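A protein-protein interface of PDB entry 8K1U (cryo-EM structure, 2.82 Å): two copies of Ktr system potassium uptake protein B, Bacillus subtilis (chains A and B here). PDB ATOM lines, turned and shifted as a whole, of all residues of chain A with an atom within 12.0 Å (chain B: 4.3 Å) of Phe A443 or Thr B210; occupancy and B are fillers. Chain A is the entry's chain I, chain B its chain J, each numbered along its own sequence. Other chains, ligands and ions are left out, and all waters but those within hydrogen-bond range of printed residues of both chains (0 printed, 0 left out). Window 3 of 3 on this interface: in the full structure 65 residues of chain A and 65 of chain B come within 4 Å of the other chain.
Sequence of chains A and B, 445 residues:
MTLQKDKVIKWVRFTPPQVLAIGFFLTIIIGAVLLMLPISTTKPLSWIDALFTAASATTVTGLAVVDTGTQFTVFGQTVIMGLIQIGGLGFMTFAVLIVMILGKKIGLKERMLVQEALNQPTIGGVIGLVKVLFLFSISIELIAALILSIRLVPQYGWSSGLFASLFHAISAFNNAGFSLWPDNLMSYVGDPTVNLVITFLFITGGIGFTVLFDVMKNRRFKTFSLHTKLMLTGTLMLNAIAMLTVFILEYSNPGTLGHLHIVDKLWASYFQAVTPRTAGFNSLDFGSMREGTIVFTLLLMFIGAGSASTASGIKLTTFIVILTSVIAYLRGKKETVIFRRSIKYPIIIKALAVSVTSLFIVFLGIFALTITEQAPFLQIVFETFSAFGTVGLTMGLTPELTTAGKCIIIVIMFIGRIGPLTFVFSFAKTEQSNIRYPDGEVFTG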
ATOM      1  N   TYR A 329       9.214  30.413 -12.705  1.00  0.00           N
ATOM      2  CA  TYR A 329       9.907  30.568 -11.429  1.00  0.00           C
ATOM      3  C   TYR A 329      10.537  31.951 -11.305  1.00  0.00           C
ATOM      4  O   TYR A 329      10.517  32.553 -10.225  1.00  0.00           O
ATOM      5  CB  TYR A 329      10.967  29.476 -11.272  1.00  0.00           C
ATOM      6  CG  TYR A 329      11.668  29.480  -9.931  1.00  0.00           C
ATOM      7  CD1 TYR A 329      11.120  28.821  -8.837  1.00  0.00           C
ATOM      8  CD2 TYR A 329      12.882  30.134  -9.759  1.00  0.00           C
ATOM      9  CE1 TYR A 329      11.758  28.819  -7.611  1.00  0.00           C
ATOM     10  CE2 TYR A 329      13.527  30.138  -8.537  1.00  0.00           C
ATOM     11  CZ  TYR A 329      12.961  29.478  -7.467  1.00  0.00           C
ATOM     12  OH  TYR A 329      13.600  29.479  -6.248  1.00  0.00           O
ATOM     13  N   ASP A 439      12.703  15.666   5.876  1.00  0.00           N
ATOM     14  CA  ASP A 439      13.199  16.690   4.968  1.00  0.00           C
ATOM     15  C   ASP A 439      14.543  17.232   5.439  1.00  0.00           C
ATOM     16  O   ASP A 439      14.758  17.463   6.632  1.00  0.00           O
ATOM     17  CB  ASP A 439      12.190  17.831   4.853  1.00  0.00           C
ATOM     18  CG  ASP A 439      10.840  17.366   4.346  1.00  0.00           C
ATOM     19  OD1 ASP A 439      10.694  16.159   4.064  1.00  0.00           O
ATOM     20  OD2 ASP A 439       9.926  18.210   4.231  1.00  0.00           O
ATOM     21  N   GLY A 440      15.445  17.434   4.491  1.00  0.00           N
ATOM     22  CA  GLY A 440      16.741  18.037   4.765  1.00  0.00           C
ATOM     23  C   GLY A 440      16.886  19.338   4.001  1.00  0.00           C
ATOM     24  O   GLY A 440      16.436  19.447   2.859  1.00  0.00           O
ATOM     25  N   GLU A 441      17.516  20.320   4.636  1.00  0.00           N
ATOM     26  CA  GLU A 441      17.686  21.645   4.056  1.00  0.00           C
ATOM     27  C   GLU A 441      19.089  21.764   3.472  1.00  0.00           C
ATOM     28  O   GLU A 441      20.083  21.618   4.191  1.00  0.00           O
ATOM     29  CB  GLU A 441      17.431  22.733   5.100  1.00  0.00           C
ATOM     30  CG  GLU A 441      17.963  22.414   6.488  1.00  0.00           C
ATOM     31  CD  GLU A 441      17.612  23.480   7.505  1.00  0.00           C
ATOM     32  OE1 GLU A 441      16.910  24.445   7.137  1.00  0.00           O
ATOM     33  OE2 GLU A 441      18.036  23.354   8.673  1.00  0.00           O
ATOM     34  N   VAL A 442      19.162  22.020   2.168  1.00  0.00           N
ATOM     35  CA  VAL A 442      20.421  22.183   1.455  1.00  0.00           C
ATOM     36  C   VAL A 442      20.315  23.437   0.596  1.00  0.00           C
ATOM     37  O   VAL A 442      19.313  23.635  -0.101  1.00  0.00           O
ATOM     38  CB  VAL A 442      20.758  20.940   0.605  1.00  0.00           C
ATOM     39  CG1 VAL A 442      19.523  20.425  -0.119  1.00  0.00           C
ATOM     40  CG2 VAL A 442      21.878  21.232  -0.380  1.00  0.00           C
ATOM     41  N   PHE A 443      21.333  24.291   0.664  1.00  0.00           N
ATOM     42  CA  PHE A 443      21.318  25.572  -0.031  1.00  0.00           C
ATOM     43  C   PHE A 443      21.839  25.374  -1.449  1.00  0.00           C
ATOM     44  O   PHE A 443      22.996  24.984  -1.641  1.00  0.00           O
ATOM     45  CB  PHE A 443      22.164  26.603   0.716  1.00  0.00           C
ATOM     46  CG  PHE A 443      21.900  26.655   2.197  1.00  0.00           C
ATOM     47  CD1 PHE A 443      20.607  26.604   2.693  1.00  0.00           C
ATOM     48  CD2 PHE A 443      22.953  26.752   3.093  1.00  0.00           C
ATOM     49  CE1 PHE A 443      20.369  26.646   4.053  1.00  0.00           C
ATOM     50  CE2 PHE A 443      22.721  26.797   4.455  1.00  0.00           C
ATOM     51  CZ  PHE A 443      21.427  26.745   4.935  1.00  0.00           C
ATOM     52  N   THR A 444      20.988  25.640  -2.436  1.00  0.00           N
ATOM     53  CA  THR A 444      21.307  25.436  -3.843  1.00  0.00           C
ATOM     54  C   THR A 444      21.296  26.756  -4.604  1.00  0.00           C
ATOM     55  O   THR A 444      20.771  26.851  -5.716  1.00  0.00           O
ATOM     56  CB  THR A 444      20.339  24.442  -4.483  1.00  0.00           C
ATOM     57  OG1 THR A 444      18.997  24.932  -4.363  1.00  0.00           O
ATOM     58  CG2 THR A 444      20.443  23.087  -3.802  1.00  0.00           C
ATOM     59  N   GLY A 445      21.877  27.793  -4.010  1.00  0.00           N
ATOM     60  CA  GLY A 445      21.939  29.096  -4.646  1.00  0.00           C
ATOM     61  C   GLY A 445      23.097  29.235  -5.614  1.00  0.00           C
ATOM     62  O   GLY A 445      23.453  28.287  -6.315  1.00  0.00           O
ATOM     63  N   GLN B 120      20.416  32.812   2.213  1.00  0.00           N
ATOM     64  CA  GLN B 120      19.866  32.114   3.368  1.00  0.00           C
ATOM     65  C   GLN B 120      18.361  31.918   3.202  1.00  0.00           C
ATOM     66  O   GLN B 120      17.693  32.749   2.579  1.00  0.00           O
ATOM     67  CB  GLN B 120      20.144  32.894   4.650  1.00  0.00           C
ATOM     68  CG  GLN B 120      20.748  32.061   5.770  1.00  0.00           C
ATOM     69  CD  GLN B 120      22.094  31.470   5.399  1.00  0.00           C
ATOM     70  OE1 GLN B 120      22.892  32.097   4.701  1.00  0.00           O
ATOM     71  NE2 GLN B 120      22.353  30.252   5.862  1.00  0.00           N
ATOM     72  N   PRO B 121      17.800  30.828   3.729  1.00  0.00           N
ATOM     73  CA  PRO B 121      16.346  30.637   3.642  1.00  0.00           C
ATOM     74  C   PRO B 121      15.594  31.369   4.742  1.00  0.00           C
ATOM     75  O   PRO B 121      14.413  31.695   4.584  1.00  0.00           O
ATOM     76  CB  PRO B 121      16.190  29.117   3.769  1.00  0.00           C
ATOM     77  CG  PRO B 121      17.346  28.706   4.613  1.00  0.00           C
ATOM     78  CD  PRO B 121      18.483  29.634   4.259  1.00  0.00           C
ATOM     79  N   LEU B 129      26.203  35.575  11.751  1.00  0.00           N
ATOM     80  CA  LEU B 129      27.036  34.892  10.768  1.00  0.00           C
ATOM     81  C   LEU B 129      28.014  35.857  10.109  1.00  0.00           C
ATOM     82  O   LEU B 129      29.152  35.483   9.803  1.00  0.00           O
ATOM     83  CB  LEU B 129      26.155  34.213   9.719  1.00  0.00           C
ATOM     84  CG  LEU B 129      26.865  33.401   8.634  1.00  0.00           C
ATOM     85  CD1 LEU B 129      27.674  32.271   9.250  1.00  0.00           C
ATOM     86  CD2 LEU B 129      25.864  32.861   7.625  1.00  0.00           C
ATOM     87  N   GLY B 208      32.407  27.520   1.893  1.00  0.00           N
ATOM     88  CA  GLY B 208      31.166  28.080   2.385  1.00  0.00           C
ATOM     89  C   GLY B 208      31.284  28.646   3.783  1.00  0.00           C
ATOM     90  O   GLY B 208      31.882  28.020   4.664  1.00  0.00           O
ATOM     91  N   PHE B 209      30.723  29.837   3.996  1.00  0.00           N
ATOM     92  CA  PHE B 209      30.754  30.444   5.322  1.00  0.00           C
ATOM     93  C   PHE B 209      29.871  29.678   6.298  1.00  0.00           C
ATOM     94  O   PHE B 209      30.194  29.571   7.486  1.00  0.00           O
ATOM     95  CB  PHE B 209      30.326  31.907   5.237  1.00  0.00           C
ATOM     96  CG  PHE B 209      31.210  32.747   4.361  1.00  0.00           C
ATOM     97  CD1 PHE B 209      32.581  32.544   4.342  1.00  0.00           C
ATOM     98  CD2 PHE B 209      30.672  33.734   3.551  1.00  0.00           C
ATOM     99  CE1 PHE B 209      33.399  33.313   3.535  1.00  0.00           C
ATOM    100  CE2 PHE B 209      31.484  34.507   2.742  1.00  0.00           C
ATOM    101  CZ  PHE B 209      32.849  34.295   2.734  1.00  0.00           C
ATOM    102  N   THR B 210      28.747  29.143   5.815  1.00  0.00           N
ATOM    103  CA  THR B 210      27.889  28.319   6.660  1.00  0.00           C
ATOM    104  C   THR B 210      28.564  26.995   7.003  1.00  0.00           C
ATOM    105  O   THR B 210      28.402  26.478   8.114  1.00  0.00           O
ATOM    106  CB  THR B 210      26.548  28.076   5.965  1.00  0.00           C
ATOM    107  OG1 THR B 210      26.033  29.319   5.473  1.00  0.00           O
ATOM    108  CG2 THR B 210      25.541  27.474   6.934  1.00  0.00           C
ATOM    109  N   VAL B 211      29.322  26.434   6.058  1.00  0.00           N
ATOM    110  CA  VAL B 211      30.043  25.190   6.313  1.00  0.00           C
ATOM    111  C   VAL B 211      31.140  25.410   7.350  1.00  0.00           C
ATOM    112  O   VAL B 211      31.324  24.590   8.258  1.00  0.00           O
ATOM    113  CB  VAL B 211      30.608  24.625   4.997  1.00  0.00           C
ATOM    114  CG1 VAL B 211      31.384  23.342   5.250  1.00  0.00           C
ATOM    115  CG2 VAL B 211      29.481  24.383   4.005  1.00  0.00           C
ATOM    116  N   LEU B 212      31.879  26.517   7.235  1.00  0.00           N
ATOM    117  CA  LEU B 212      32.913  26.830   8.217  1.00  0.00           C
ATOM    118  C   LEU B 212      32.312  27.088   9.592  1.00  0.00           C
ATOM    119  O   LEU B 212      32.882  26.682  10.612  1.00  0.00           O
ATOM    120  CB  LEU B 212      33.729  28.037   7.757  1.00  0.00           C
ATOM    121  CG  LEU B 212      34.649  27.812   6.559  1.00  0.00           C
ATOM    122  CD1 LEU B 212      35.278  29.123   6.121  1.00  0.00           C
ATOM    123  CD2 LEU B 212      35.720  26.785   6.895  1.00  0.00           C
ATOM    124  N   PHE B 213      31.166  27.771   9.641  1.00  0.00           N
ATOM    125  CA  PHE B 213      30.510  28.039  10.916  1.00  0.00           C
ATOM    126  C   PHE B 213      30.023  26.757  11.582  1.00  0.00           C
ATOM    127  O   PHE B 213      30.001  26.671  12.814  1.00  0.00           O
ATOM    128  CB  PHE B 213      29.346  29.010  10.712  1.00  0.00           C
ATOM    129  CG  PHE B 213      28.643  29.393  11.983  1.00  0.00           C
ATOM    130  CD1 PHE B 213      29.197  30.327  12.842  1.00  0.00           C
ATOM    131  CD2 PHE B 213      27.422  28.826  12.313  1.00  0.00           C
ATOM    132  CE1 PHE B 213      28.552  30.684  14.012  1.00  0.00           C
ATOM    133  CE2 PHE B 213      26.771  29.178  13.482  1.00  0.00           C
ATOM    134  CZ  PHE B 213      27.337  30.109  14.332  1.00  0.00           C
ATOM    135  N   ASP B 214      29.634  25.754  10.790  1.00  0.00           N
ATOM    136  CA  ASP B 214      29.160  24.499  11.363  1.00  0.00           C
ATOM    137  C   ASP B 214      30.313  23.678  11.929  1.00  0.00           C
ATOM    138  O   ASP B 214      30.164  23.022  12.966  1.00  0.00           O
ATOM    139  CB  ASP B 214      28.393  23.702  10.307  1.00  0.00           C
ATOM    140  CG  ASP B 214      27.517  22.620  10.912  1.00  0.00           C
ATOM    141  OD1 ASP B 214      27.409  22.563  12.155  1.00  0.00           O
ATOM    142  OD2 ASP B 214      26.934  21.828  10.143  1.00  0.00           O
ATOM    143  N   HIS B 227      23.753  20.208   4.322  1.00  0.00           N
ATOM    144  CA  HIS B 227      24.583  21.050   3.465  1.00  0.00           C
ATOM    145  C   HIS B 227      26.061  20.912   3.813  1.00  0.00           C
ATOM    146  O   HIS B 227      26.914  20.899   2.918  1.00  0.00           O
ATOM    147  CB  HIS B 227      24.139  22.508   3.581  1.00  0.00           C
ATOM    148  CG  HIS B 227      24.888  23.443   2.683  1.00  0.00           C
ATOM    149  ND1 HIS B 227      24.481  23.724   1.397  1.00  0.00           N
ATOM    150  CD2 HIS B 227      26.020  24.158   2.884  1.00  0.00           C
ATOM    151  CE1 HIS B 227      25.328  24.575   0.846  1.00  0.00           C
ATOM    152  NE2 HIS B 227      26.272  24.853   1.727  1.00  0.00           N
ATOM    153  N   SER B 307      27.483  27.652  -1.280  1.00  0.00           N
ATOM    154  CA  SER B 307      26.406  28.568  -1.641  1.00  0.00           C
ATOM    155  C   SER B 307      26.696  29.982  -1.156  1.00  0.00           C
ATOM    156  O   SER B 307      26.446  30.955  -1.877  1.00  0.00           O
ATOM    157  CB  SER B 307      25.078  28.068  -1.079  1.00  0.00           C
ATOM    158  OG  SER B 307      24.016  28.936  -1.434  1.00  0.00           O
ATOM    159  N   THR B 317      26.546  21.956  -4.303  1.00  0.00           N
ATOM    160  CA  THR B 317      25.275  21.411  -3.842  1.00  0.00           C
ATOM    161  C   THR B 317      24.215  21.456  -4.934  1.00  0.00           C
ATOM    162  O   THR B 317      23.358  20.569  -4.998  1.00  0.00           O
ATOM    163  CB  THR B 317      24.794  22.170  -2.607  1.00  0.00           C
ATOM    164  OG1 THR B 317      24.738  23.572  -2.895  1.00  0.00           O
ATOM    165  CG2 THR B 317      25.738  21.932  -1.439  1.00  0.00           C
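A ring nitrogen (ND1) of His B227 is in hydrogen-bond range of the backbone NH (N) of Phe A443 (3.3 Å).
The side-chain hydroxyl (OG1) of Thr B317 lies within hydrogen-bond range of the backbone carbonyl oxygen (O) of Phe A443 (2.6 Å).
Glu A441 touches His B227 (O to N, 3.9 Å).
Thr B317 touches Val A442 (CB to CG2, 3.8 Å).
Phe A443 touches Gln B120.
Pro B121 touches Phe A443.
CG2 of Thr B210 touches CE2 of Phe A443, at 3.8 Å.
CB of Phe A443 touches OG of Ser B307, 3.7 Å away.
N of Gly A445 touches OG of Ser B307 (3.5 Å).
Phe A443 touches six residues of chain B.
Of chain A, only Phe A443 (3.8 Å) comes within 4 Å of Thr B210.
Printed residues of chain A within 4 Å of Pro B121: Phe A443.
No residue of chain A comes within 4 Å of Gly B208.
No residue of chain A comes within 4 Å of Phe B209.
No residue of chain A comes within 4 Å of Phe B213.
No residue of chain A comes within 4 Å of Asp B214.
Of the printed residues of chain A, Ser B307 touches Phe A443 (3.7 Å) and Gly A445 (3.5 Å).
Of the printed residues of chain B, Val A442 touches Thr B317.
Printed residues of chain B within 4 Å of Gly A445: Ser B307 (3.5 Å).
Thr A444 touches none of the printed residues of chain B.
The nearest printed residue of chain A that does not touch Thr B317 is Thr A444 (4.02 Å).
Of the 8 printed residues of chain A, 4 touch a printed residue of chain B.
Printed residues of chain A that touch a printed residue of chain B: Glu A441, Val A442, Phe A443 and Gly A445.
Hydrophobic or aromatic side chains of chain A within 4 Å of the printed part of chain B: Val A442 and Phe A443.
Of the 13 printed residues of chain B, 6 touch a printed residue of chain A.
Printed residues of chain B that touch a printed residue of chain A: Gln B120, Pro B121, Thr B210, His B227, Ser B307 and Thr B317.
Hydrophobic or aromatic side chains of chain B within 4 Å of the printed part of chain A: Pro B121 and His B227.
Among the printed residues, 9 pairs touch across the chains.
Among the printed residues, no Asp or Glu carboxylate lies within 4 Å of a Lys or Arg side-chain nitrogen of the other chain.
No position is printed for both chains.
Of the 9 pairs that touch across the chains among the printed residues, none has its exchanged pair printed and touching as well.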
